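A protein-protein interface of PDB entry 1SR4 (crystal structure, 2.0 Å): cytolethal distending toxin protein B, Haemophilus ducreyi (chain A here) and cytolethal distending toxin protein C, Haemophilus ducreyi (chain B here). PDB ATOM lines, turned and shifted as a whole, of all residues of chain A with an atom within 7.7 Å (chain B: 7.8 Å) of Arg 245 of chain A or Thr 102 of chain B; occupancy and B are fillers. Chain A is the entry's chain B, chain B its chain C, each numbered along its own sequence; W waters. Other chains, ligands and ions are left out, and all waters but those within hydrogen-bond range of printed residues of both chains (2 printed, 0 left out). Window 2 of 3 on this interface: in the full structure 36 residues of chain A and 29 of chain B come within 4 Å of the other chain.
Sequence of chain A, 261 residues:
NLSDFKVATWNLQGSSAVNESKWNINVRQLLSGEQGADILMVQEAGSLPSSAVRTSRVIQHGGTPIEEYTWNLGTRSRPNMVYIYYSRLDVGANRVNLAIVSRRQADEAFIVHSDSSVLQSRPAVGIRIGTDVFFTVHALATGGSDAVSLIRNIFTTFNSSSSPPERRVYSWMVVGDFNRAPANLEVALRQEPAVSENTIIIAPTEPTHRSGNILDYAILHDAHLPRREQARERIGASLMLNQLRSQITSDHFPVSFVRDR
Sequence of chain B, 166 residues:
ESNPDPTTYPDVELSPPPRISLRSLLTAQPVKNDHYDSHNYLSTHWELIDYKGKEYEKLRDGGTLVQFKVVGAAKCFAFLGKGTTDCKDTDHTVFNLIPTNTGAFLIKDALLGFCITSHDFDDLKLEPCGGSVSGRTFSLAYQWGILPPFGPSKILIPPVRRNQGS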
ATOM      1  N   ILE A  25      -1.598  -4.009  11.331  1.00  0.00           N
ATOM      2  CA  ILE A  25      -2.433  -4.030  10.142  1.00  0.00           C
ATOM      3  C   ILE A  25      -1.677  -4.780   9.035  1.00  0.00           C
ATOM      4  O   ILE A  25      -2.022  -5.918   8.694  1.00  0.00           O
ATOM      5  CB  ILE A  25      -2.772  -2.600   9.659  1.00  0.00           C
ATOM      6  CG1 ILE A  25      -3.664  -1.914  10.702  1.00  0.00           C
ATOM      7  CG2 ILE A  25      -3.462  -2.639   8.262  1.00  0.00           C
ATOM      8  CD1 ILE A  25      -3.918  -0.442  10.422  1.00  0.00           C
ATOM      9  N   ASN A  26      -0.607  -4.181   8.513  1.00  0.00           N
ATOM     10  CA  ASN A  26       0.120  -4.797   7.404  1.00  0.00           C
ATOM     11  C   ASN A  26       1.113  -5.934   7.687  1.00  0.00           C
ATOM     12  O   ASN A  26       1.063  -6.978   7.020  1.00  0.00           O
ATOM     13  CB  ASN A  26       0.816  -3.704   6.598  1.00  0.00           C
ATOM     14  CG  ASN A  26      -0.156  -2.662   6.081  1.00  0.00           C
ATOM     15  OD1 ASN A  26      -0.065  -1.486   6.427  1.00  0.00           O
ATOM     16  ND2 ASN A  26      -1.101  -3.091   5.254  1.00  0.00           N
ATOM     17  N   GLN A  29      -0.653  -9.156   8.218  1.00  0.00           N
ATOM     18  CA  GLN A  29      -1.194  -9.740   6.997  1.00  0.00           C
ATOM     19  C   GLN A  29      -0.115 -10.354   6.095  1.00  0.00           C
ATOM     20  O   GLN A  29      -0.367 -11.351   5.410  1.00  0.00           O
ATOM     21  CB  GLN A  29      -2.030  -8.680   6.238  1.00  0.00           C
ATOM     22  CG  GLN A  29      -3.358  -8.365   6.956  1.00  0.00           C
ATOM     23  CD  GLN A  29      -4.113  -7.140   6.415  1.00  0.00           C
ATOM     24  OE1 GLN A  29      -3.819  -6.638   5.327  1.00  0.00           O
ATOM     25  NE2 GLN A  29      -5.112  -6.668   7.185  1.00  0.00           N
ATOM     26  N   SER A  32       0.522 -14.004   7.474  1.00  0.00           N
ATOM     27  CA  SER A  32      -0.505 -15.029   7.631  1.00  0.00           C
ATOM     28  C   SER A  32      -0.910 -15.818   6.410  1.00  0.00           C
ATOM     29  O   SER A  32      -0.495 -15.528   5.286  1.00  0.00           O
ATOM     30  CB  SER A  32      -1.750 -14.429   8.276  1.00  0.00           C
ATOM     31  OG  SER A  32      -2.278 -13.407   7.481  1.00  0.00           O
ATOM     32  N   GLY A  33      -1.716 -16.846   6.662  1.00  0.00           N
ATOM     33  CA  GLY A  33      -2.215 -17.678   5.592  1.00  0.00           C
ATOM     34  C   GLY A  33      -1.169 -18.591   5.005  1.00  0.00           C
ATOM     35  O   GLY A  33       0.003 -18.528   5.367  1.00  0.00           O
ATOM     36  N   GLU A  34      -1.619 -19.445   4.093  1.00  0.00           N
ATOM     37  CA  GLU A  34      -0.780 -20.409   3.391  1.00  0.00           C
ATOM     38  C   GLU A  34       0.341 -19.746   2.600  1.00  0.00           C
ATOM     39  O   GLU A  34       1.386 -20.352   2.384  1.00  0.00           O
ATOM     40  CB  GLU A  34      -1.642 -21.226   2.406  1.00  0.00           C
ATOM     41  CG  GLU A  34      -2.246 -22.526   2.952  1.00  0.00           C
ATOM     42  CD  GLU A  34      -3.225 -23.179   1.962  1.00  0.00           C
ATOM     43  OE1 GLU A  34      -2.962 -23.127   0.744  1.00  0.00           O
ATOM     44  OE2 GLU A  34      -4.253 -23.750   2.400  1.00  0.00           O
ATOM     45  N   GLN A  35       0.117 -18.516   2.141  1.00  0.00           N
ATOM     46  CA  GLN A  35       1.121 -17.820   1.334  1.00  0.00           C
ATOM     47  C   GLN A  35       1.905 -16.746   2.101  1.00  0.00           C
ATOM     48  O   GLN A  35       2.623 -15.946   1.510  1.00  0.00           O
ATOM     49  CB  GLN A  35       0.447 -17.208   0.101  1.00  0.00           C
ATOM     50  CG  GLN A  35      -0.341 -18.251  -0.732  1.00  0.00           C
ATOM     51  CD  GLN A  35      -1.145 -17.644  -1.889  1.00  0.00           C
ATOM     52  OE1 GLN A  35      -0.630 -17.456  -2.987  1.00  0.00           O
ATOM     53  NE2 GLN A  35      -2.409 -17.335  -1.634  1.00  0.00           N
ATOM     54  N   MET A 240       3.645  -7.966  -3.165  1.00  0.00           N
ATOM     55  CA  MET A 240       2.922  -9.006  -2.417  1.00  0.00           C
ATOM     56  C   MET A 240       1.454  -8.645  -2.176  1.00  0.00           C
ATOM     57  O   MET A 240       0.961  -8.677  -1.047  1.00  0.00           O
ATOM     58  CB  MET A 240       3.616  -9.263  -1.069  1.00  0.00           C
ATOM     59  CG  MET A 240       3.128 -10.531  -0.361  1.00  0.00           C
ATOM     60  SD  MET A 240       4.210 -10.881   1.014  1.00  0.00           S
ATOM     61  CE  MET A 240       4.121 -12.662   1.109  1.00  0.00           C
ATOM     62  N   LEU A 241       0.749  -8.346  -3.257  1.00  0.00           N
ATOM     63  CA  LEU A 241      -0.634  -7.920  -3.155  1.00  0.00           C
ATOM     64  C   LEU A 241      -1.604  -9.004  -2.745  1.00  0.00           C
ATOM     65  O   LEU A 241      -2.693  -8.706  -2.268  1.00  0.00           O
ATOM     66  CB  LEU A 241      -1.069  -7.284  -4.474  1.00  0.00           C
ATOM     67  CG  LEU A 241      -0.166  -6.152  -4.983  1.00  0.00           C
ATOM     68  CD1 LEU A 241      -0.655  -5.704  -6.353  1.00  0.00           C
ATOM     69  CD2 LEU A 241      -0.163  -4.988  -3.998  1.00  0.00           C
ATOM     70  N   ASN A 242      -1.216 -10.264  -2.917  1.00  0.00           N
ATOM     71  CA  ASN A 242      -2.092 -11.370  -2.541  1.00  0.00           C
ATOM     72  C   ASN A 242      -2.287 -11.476  -1.018  1.00  0.00           C
ATOM     73  O   ASN A 242      -3.181 -12.180  -0.546  1.00  0.00           O
ATOM     74  CB  ASN A 242      -1.543 -12.684  -3.110  1.00  0.00           C
ATOM     75  CG  ASN A 242      -0.118 -12.950  -2.701  1.00  0.00           C
ATOM     76  OD1 ASN A 242       0.764 -12.108  -2.876  1.00  0.00           O
ATOM     77  ND2 ASN A 242       0.121 -14.132  -2.159  1.00  0.00           N
ATOM     78  N   GLN A 243      -1.469 -10.752  -0.260  1.00  0.00           N
ATOM     79  CA  GLN A 243      -1.567 -10.789   1.195  1.00  0.00           C
ATOM     80  C   GLN A 243      -2.404  -9.659   1.821  1.00  0.00           C
ATOM     81  O   GLN A 243      -2.856  -9.784   2.967  1.00  0.00           O
ATOM     82  CB  GLN A 243      -0.167 -10.757   1.807  1.00  0.00           C
ATOM     83  CG  GLN A 243       0.657 -12.025   1.611  1.00  0.00           C
ATOM     84  CD  GLN A 243      -0.034 -13.279   2.139  1.00  0.00           C
ATOM     85  OE1 GLN A 243      -0.620 -14.038   1.372  1.00  0.00           O
ATOM     86  NE2 GLN A 243       0.033 -13.496   3.453  1.00  0.00           N
ATOM     87  N   LEU A 244      -2.657  -8.595   1.057  1.00  0.00           N
ATOM     88  CA  LEU A 244      -3.383  -7.433   1.571  1.00  0.00           C
ATOM     89  C   LEU A 244      -4.903  -7.561   1.742  1.00  0.00           C
ATOM     90  O   LEU A 244      -5.589  -8.143   0.906  1.00  0.00           O
ATOM     91  CB  LEU A 244      -3.067  -6.212   0.692  1.00  0.00           C
ATOM     92  CG  LEU A 244      -1.580  -6.024   0.361  1.00  0.00           C
ATOM     93  CD1 LEU A 244      -1.388  -4.746  -0.436  1.00  0.00           C
ATOM     94  CD2 LEU A 244      -0.757  -5.960   1.640  1.00  0.00           C
ATOM     95  N   ARG A 245      -5.403  -7.006   2.846  1.00  0.00           N
ATOM     96  CA  ARG A 245      -6.836  -6.992   3.164  1.00  0.00           C
ATOM     97  C   ARG A 245      -7.133  -5.588   3.707  1.00  0.00           C
ATOM     98  O   ARG A 245      -8.216  -5.329   4.208  1.00  0.00           O
ATOM     99  CB  ARG A 245      -7.148  -8.006   4.259  1.00  0.00           C
ATOM    100  CG  ARG A 245      -6.550  -9.404   4.038  1.00  0.00           C
ATOM    101  CD  ARG A 245      -7.261 -10.150   2.935  1.00  0.00           C
ATOM    102  NE  ARG A 245      -6.824 -11.555   2.856  1.00  0.00           N
ATOM    103  CZ  ARG A 245      -5.919 -12.015   1.992  1.00  0.00           C
ATOM    104  NH1 ARG A 245      -5.337 -11.193   1.121  1.00  0.00           N
ATOM    105  NH2 ARG A 245      -5.601 -13.305   1.989  1.00  0.00           N
ATOM    106  N   SER A 246      -6.148  -4.694   3.580  1.00  0.00           N
ATOM    107  CA  SER A 246      -6.230  -3.327   4.096  1.00  0.00           C
ATOM    108  C   SER A 246      -5.378  -2.354   3.296  1.00  0.00           C
ATOM    109  O   SER A 246      -4.578  -2.749   2.454  1.00  0.00           O
ATOM    110  CB  SER A 246      -5.666  -3.268   5.526  1.00  0.00           C
ATOM    111  OG  SER A 246      -6.382  -4.083   6.441  1.00  0.00           O
ATOM    112  N   GLN A 247      -5.538  -1.075   3.616  1.00  0.00           N
ATOM    113  CA  GLN A 247      -4.712  -0.031   3.033  1.00  0.00           C
ATOM    114  C   GLN A 247      -3.271  -0.382   3.460  1.00  0.00           C
ATOM    115  O   GLN A 247      -3.058  -0.971   4.540  1.00  0.00           O
ATOM    116  CB  GLN A 247      -5.094   1.319   3.649  1.00  0.00           C
ATOM    117  CG  GLN A 247      -4.072   2.446   3.475  1.00  0.00           C
ATOM    118  CD  GLN A 247      -3.880   2.844   2.023  1.00  0.00           C
ATOM    119  OE1 GLN A 247      -3.603   1.991   1.165  1.00  0.00           O
ATOM    120  NE2 GLN A 247      -4.019   4.140   1.733  1.00  0.00           N
ATOM    121  N   ILE A 248      -2.295  -0.065   2.611  1.00  0.00           N
ATOM    122  CA  ILE A 248      -0.886  -0.280   2.944  1.00  0.00           C
ATOM    123  C   ILE A 248      -0.538   1.018   3.647  1.00  0.00           C
ATOM    124  O   ILE A 248      -0.644   2.090   3.049  1.00  0.00           O
ATOM    125  CB  ILE A 248      -0.009  -0.456   1.683  1.00  0.00           C
ATOM    126  CG1 ILE A 248      -0.450  -1.709   0.925  1.00  0.00           C
ATOM    127  CG2 ILE A 248       1.473  -0.619   2.081  1.00  0.00           C
ATOM    128  CD1 ILE A 248       0.456  -2.063  -0.236  1.00  0.00           C
ATOM    129  N   LEU B  25     -17.905  -3.684   7.085  1.00  0.00           N
ATOM    130  CA  LEU B  25     -17.894  -4.752   6.097  1.00  0.00           C
ATOM    131  C   LEU B  25     -19.301  -5.245   5.814  1.00  0.00           C
ATOM    132  O   LEU B  25     -19.529  -5.983   4.856  1.00  0.00           O
ATOM    133  CB  LEU B  25     -17.014  -5.914   6.544  1.00  0.00           C
ATOM    134  CG  LEU B  25     -15.531  -5.550   6.617  1.00  0.00           C
ATOM    135  CD1 LEU B  25     -14.720  -6.846   6.669  1.00  0.00           C
ATOM    136  CD2 LEU B  25     -15.127  -4.719   5.388  1.00  0.00           C
ATOM    137  N   PRO B  99      -7.137  -7.007  15.768  1.00  0.00           N
ATOM    138  CA  PRO B  99      -6.943  -7.776  14.534  1.00  0.00           C
ATOM    139  C   PRO B  99      -7.726  -9.091  14.566  1.00  0.00           C
ATOM    140  O   PRO B  99      -8.086  -9.585  15.637  1.00  0.00           O
ATOM    141  CB  PRO B  99      -5.424  -8.005  14.491  1.00  0.00           C
ATOM    142  CG  PRO B  99      -5.062  -8.131  15.945  1.00  0.00           C
ATOM    143  CD  PRO B  99      -5.934  -7.051  16.628  1.00  0.00           C
ATOM    144  N   THR B 100      -7.977  -9.651  13.384  1.00  0.00           N
ATOM    145  CA  THR B 100      -8.720 -10.908  13.250  1.00  0.00           C
ATOM    146  C   THR B 100      -8.021 -11.829  12.252  1.00  0.00           C
ATOM    147  O   THR B 100      -7.056 -11.420  11.589  1.00  0.00           O
ATOM    148  CB  THR B 100     -10.142 -10.676  12.704  1.00  0.00           C
ATOM    149  OG1 THR B 100     -10.063 -10.281  11.332  1.00  0.00           O
ATOM    150  CG2 THR B 100     -10.860  -9.609  13.497  1.00  0.00           C
ATOM    151  N   ASN B 101      -8.519 -13.059  12.126  1.00  0.00           N
ATOM    152  CA  ASN B 101      -7.926 -14.005  11.185  1.00  0.00           C
ATOM    153  C   ASN B 101      -8.294 -13.708   9.736  1.00  0.00           C
ATOM    154  O   ASN B 101      -7.857 -14.434   8.829  1.00  0.00           O
ATOM    155  CB  ASN B 101      -8.314 -15.463  11.530  1.00  0.00           C
ATOM    156  CG  ASN B 101      -9.829 -15.727  11.489  1.00  0.00           C
ATOM    157  OD1 ASN B 101     -10.653 -14.806  11.469  1.00  0.00           O
ATOM    158  ND2 ASN B 101     -10.196 -17.014  11.490  1.00  0.00           N
ATOM    159  N   THR B 102      -9.095 -12.670   9.493  1.00  0.00           N
ATOM    160  CA  THR B 102      -9.448 -12.353   8.105  1.00  0.00           C
ATOM    161  C   THR B 102      -8.852 -11.052   7.577  1.00  0.00           C
ATOM    162  O   THR B 102      -8.890 -10.807   6.364  1.00  0.00           O
ATOM    163  CB  THR B 102     -10.969 -12.233   7.874  1.00  0.00           C
ATOM    164  OG1 THR B 102     -11.448 -11.023   8.465  1.00  0.00           O
ATOM    165  CG2 THR B 102     -11.713 -13.434   8.466  1.00  0.00           C
ATOM    166  N   GLY B 103      -8.311 -10.218   8.463  1.00  0.00           N
ATOM    167  CA  GLY B 103      -7.775  -8.942   8.009  1.00  0.00           C
ATOM    168  C   GLY B 103      -8.768  -7.826   8.316  1.00  0.00           C
ATOM    169  O   GLY B 103      -8.467  -6.644   8.162  1.00  0.00           O
ATOM    170  N   ALA B 104      -9.984  -8.208   8.697  1.00  0.00           N
ATOM    171  CA  ALA B 104     -10.979  -7.231   9.101  1.00  0.00           C
ATOM    172  C   ALA B 104     -10.576  -6.882  10.535  1.00  0.00           C
ATOM    173  O   ALA B 104      -9.801  -7.621  11.160  1.00  0.00           O
ATOM    174  CB  ALA B 104     -12.357  -7.856   9.108  1.00  0.00           C
ATOM    175  N   PHE B 105     -11.114  -5.782  11.051  1.00  0.00           N
ATOM    176  CA  PHE B 105     -10.835  -5.365  12.416  1.00  0.00           C
ATOM    177  C   PHE B 105     -12.119  -5.162  13.183  1.00  0.00           C
ATOM    178  O   PHE B 105     -13.166  -4.827  12.601  1.00  0.00           O
ATOM    179  CB  PHE B 105     -10.075  -4.027  12.447  1.00  0.00           C
ATOM    180  CG  PHE B 105      -8.682  -4.128  11.926  1.00  0.00           C
ATOM    181  CD1 PHE B 105      -7.639  -4.499  12.776  1.00  0.00           C
ATOM    182  CD2 PHE B 105      -8.428  -3.957  10.570  1.00  0.00           C
ATOM    183  CE1 PHE B 105      -6.347  -4.710  12.275  1.00  0.00           C
ATOM    184  CE2 PHE B 105      -7.133  -4.167  10.064  1.00  0.00           C
ATOM    185  CZ  PHE B 105      -6.101  -4.544  10.921  1.00  0.00           C
ATOM    186  N   PHE B 138     -17.104 -13.273  15.229  1.00  0.00           N
ATOM    187  CA  PHE B 138     -18.034 -12.169  15.050  1.00  0.00           C
ATOM    188  C   PHE B 138     -18.596 -12.031  13.632  1.00  0.00           C
ATOM    189  O   PHE B 138     -17.896 -12.281  12.652  1.00  0.00           O
ATOM    190  CB  PHE B 138     -17.298 -10.870  15.424  1.00  0.00           C
ATOM    191  CG  PHE B 138     -16.852 -10.815  16.868  1.00  0.00           C
ATOM    192  CD1 PHE B 138     -17.702 -10.314  17.855  1.00  0.00           C
ATOM    193  CD2 PHE B 138     -15.592 -11.267  17.239  1.00  0.00           C
ATOM    194  CE1 PHE B 138     -17.297 -10.260  19.195  1.00  0.00           C
ATOM    195  CE2 PHE B 138     -15.176 -11.219  18.580  1.00  0.00           C
ATOM    196  CZ  PHE B 138     -16.026 -10.715  19.555  1.00  0.00           C
ATOM    197  N   LEU B 140     -20.277  -9.844  10.388  1.00  0.00           N
ATOM    198  CA  LEU B 140     -19.822  -8.635   9.697  1.00  0.00           C
ATOM    199  C   LEU B 140     -20.265  -7.335  10.365  1.00  0.00           C
ATOM    200  O   LEU B 140     -19.644  -6.294  10.175  1.00  0.00           O
ATOM    201  CB  LEU B 140     -20.310  -8.648   8.238  1.00  0.00           C
ATOM    202  CG  LEU B 140     -19.775  -9.797   7.371  1.00  0.00           C
ATOM    203  CD1 LEU B 140     -20.581  -9.911   6.068  1.00  0.00           C
ATOM    204  CD2 LEU B 140     -18.298  -9.530   7.051  1.00  0.00           C
ATOM    205  N   GLN B 143     -17.423  -6.016  12.106  1.00  0.00           N
ATOM    206  CA  GLN B 143     -16.210  -5.912  11.311  1.00  0.00           C
ATOM    207  C   GLN B 143     -16.035  -4.654  10.500  1.00  0.00           C
ATOM    208  O   GLN B 143     -16.972  -4.165   9.883  1.00  0.00           O
ATOM    209  CB  GLN B 143     -16.132  -7.110  10.375  1.00  0.00           C
ATOM    210  CG  GLN B 143     -16.198  -8.474  11.080  1.00  0.00           C
ATOM    211  CD  GLN B 143     -16.065  -9.596  10.078  1.00  0.00           C
ATOM    212  OE1 GLN B 143     -15.308  -9.480   9.111  1.00  0.00           O
ATOM    213  NE2 GLN B 143     -16.781 -10.695  10.304  1.00  0.00           N
ATOM    214  N   TRP B 144     -14.798  -4.176  10.472  1.00  0.00           N
ATOM    215  CA  TRP B 144     -14.433  -2.962   9.769  1.00  0.00           C
ATOM    216  C   TRP B 144     -13.244  -3.141   8.834  1.00  0.00           C
ATOM    217  O   TRP B 144     -12.300  -3.875   9.138  1.00  0.00           O
ATOM    218  CB  TRP B 144     -14.106  -1.890  10.808  1.00  0.00           C
ATOM    219  CG  TRP B 144     -15.313  -1.605  11.640  1.00  0.00           C
ATOM    220  CD1 TRP B 144     -15.727  -2.274  12.757  1.00  0.00           C
ATOM    221  CD2 TRP B 144     -16.353  -0.688  11.309  1.00  0.00           C
ATOM    222  NE1 TRP B 144     -16.979  -1.832  13.134  1.00  0.00           N
ATOM    223  CE2 TRP B 144     -17.386  -0.860  12.261  1.00  0.00           C
ATOM    224  CE3 TRP B 144     -16.517   0.261  10.291  1.00  0.00           C
ATOM    225  CZ2 TRP B 144     -18.573  -0.114  12.224  1.00  0.00           C
ATOM    226  CZ3 TRP B 144     -17.696   0.999  10.249  1.00  0.00           C
ATOM    227  CH2 TRP B 144     -18.709   0.806  11.210  1.00  0.00           C
ATOM    228  N   GLY B 145     -13.286  -2.459   7.699  1.00  0.00           N
ATOM    229  CA  GLY B 145     -12.167  -2.527   6.778  1.00  0.00           C
ATOM    230  C   GLY B 145     -11.413  -1.211   6.850  1.00  0.00           C
ATOM    231  O   GLY B 145     -12.028  -0.147   6.779  1.00  0.00           O
ATOM    232  N   ILE B 146     -10.100  -1.270   7.055  1.00  0.00           N
ATOM    233  CA  ILE B 146      -9.263  -0.066   7.086  1.00  0.00           C
ATOM    234  C   ILE B 146      -8.714  -0.126   5.666  1.00  0.00           C
ATOM    235  O   ILE B 146      -7.757  -0.843   5.391  1.00  0.00           O
ATOM    236  CB  ILE B 146      -8.119  -0.189   8.128  1.00  0.00           C
ATOM    237  CG1 ILE B 146      -8.674  -0.084   9.558  1.00  0.00           C
ATOM    238  CG2 ILE B 146      -7.138   0.988   7.984  1.00  0.00           C
ATOM    239  CD1 ILE B 146      -9.751  -1.065   9.873  1.00  0.00           C
ATOM    240  N   LEU B 147      -9.339   0.629   4.775  1.00  0.00           N
ATOM    241  CA  LEU B 147      -9.026   0.565   3.349  1.00  0.00           C
ATOM    242  C   LEU B 147      -8.489   1.827   2.688  1.00  0.00           C
ATOM    243  O   LEU B 147      -8.445   2.894   3.300  1.00  0.00           O
ATOM    244  CB  LEU B 147     -10.307   0.117   2.615  1.00  0.00           C
ATOM    245  CG  LEU B 147     -10.866  -1.254   3.047  1.00  0.00           C
ATOM    246  CD1 LEU B 147     -12.328  -1.415   2.646  1.00  0.00           C
ATOM    247  CD2 LEU B 147     -10.030  -2.359   2.411  1.00  0.00           C
ATOM    248  N   PRO B 148      -8.067   1.713   1.410  1.00  0.00           N
ATOM    249  CA  PRO B 148      -7.550   2.893   0.709  1.00  0.00           C
ATOM    250  C   PRO B 148      -8.645   3.974   0.756  1.00  0.00           C
ATOM    251  O   PRO B 148      -9.840   3.667   0.791  1.00  0.00           O
ATOM    252  CB  PRO B 148      -7.292   2.369  -0.710  1.00  0.00           C
ATOM    253  CG  PRO B 148      -6.928   0.897  -0.473  1.00  0.00           C
ATOM    254  CD  PRO B 148      -7.964   0.499   0.570  1.00  0.00           C
HETATM  255  O   HOH W   1      -8.016 -12.874   4.913  1.00  0.00           O
HETATM  256  O   HOH W   2      -9.145  -4.273   6.612  1.00  0.00           O
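Of the 16 printed residues of chain A, 5 touch a printed residue of chain B. Hydrophobic or aromatic side chains of chain A within 4 Å of the printed part of chain B: Ile 25. Among the printed residues, no Asp or Glu carboxylate lies within 4 Å of a Lys or Arg side-chain nitrogen of the other chain.
The side-chain amide nitrogen of Gln 29 of chain A is in hydrogen-bond range of the backbone carbonyl oxygen of Gly 103 of chain B, 3.5 Å away. N of Gln 247 of chain A sits at hydrogen-bond distance from O of Ile 146 of chain B (2.9 Å).
Among the printed residues, merely in contact across the chains: Ser 246 of chain A with Ile 146 of chain B, Gln 247 of chain A with Leu 147 of chain B, Arg 245 of chain A with Thr 102 of chain B, Ile 25 of chain A with Phe 105 of chain B, Ser 246 of chain A with Phe 105 of chain B, Ser 246 of chain A with Gly 103 of chain B, Gln 247 of chain A with Pro 148 of chain B, Arg 245 of chain A with Gly 103 of chain B and Arg 245 of chain A with Leu 147 of chain B.
Gln 35 of chain A touches none of the printed residues of chain B. Arg 245 of chain A touches just these residues of chain B: Thr 102, Gly 103 and Leu 147. Printed residues of chain B within 4 Å of Gln 247 of chain A: Ile 146 (2.9 Å), Leu 147 (3.6 Å) and Pro 148 (3.7 Å). Thr 102 of chain B touches one residue of chain A. Of the printed residues of chain A, Gly 103 of chain B touches Gln 29, Arg 245 and Ser 246. Ala 104 of chain B touches none of the printed residues of chain A. Printed residues of chain A within 4 Å of Leu 147 of chain B: Arg 245 and Gln 247. Printed residues of chain A within 4 Å of Pro 148 of chain B: Gln 247.
Water W1 bridges O of Thr 102 of chain B (2.7 Å) and NE of Arg 245 of chain A (2.7 Å). Water W2 lies within hydrogen-bond range of OG of Ser 246 of chain A, O of Arg 245 of chain A, O of Gly 103 of chain B and N of Ile 146 of chain B.
The side-chain hydroxyl (OG) of Ser 32 of chain A lies within hydrogen-bond range of the backbone carbonyl oxygen (O) of Gln 29 of chain A, at 3.5 Å. The backbone NH of Arg 245 of chain A is in hydrogen-bond range of the side-chain amide oxygen of Gln 29 of chain A (3.0 Å). The side-chain amide nitrogen (NE2) of Gln 29 of chain A sits at hydrogen-bond distance from the side-chain hydroxyl (OG) of Ser 246 of chain A (3.0 Å). The guanidinium group (NH1) of Arg 245 of chain A lies close to the backbone carbonyl oxygen (O) of Gln 243 of chain A, at 3.4 Å. OG1 of Thr 100 of chain B lies within hydrogen-bond range of N of Gly 103 of chain B (3.4 Å). OG1 of Thr 102 of chain B lies within hydrogen-bond range of N of Ala 104 of chain B (3.2 Å).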
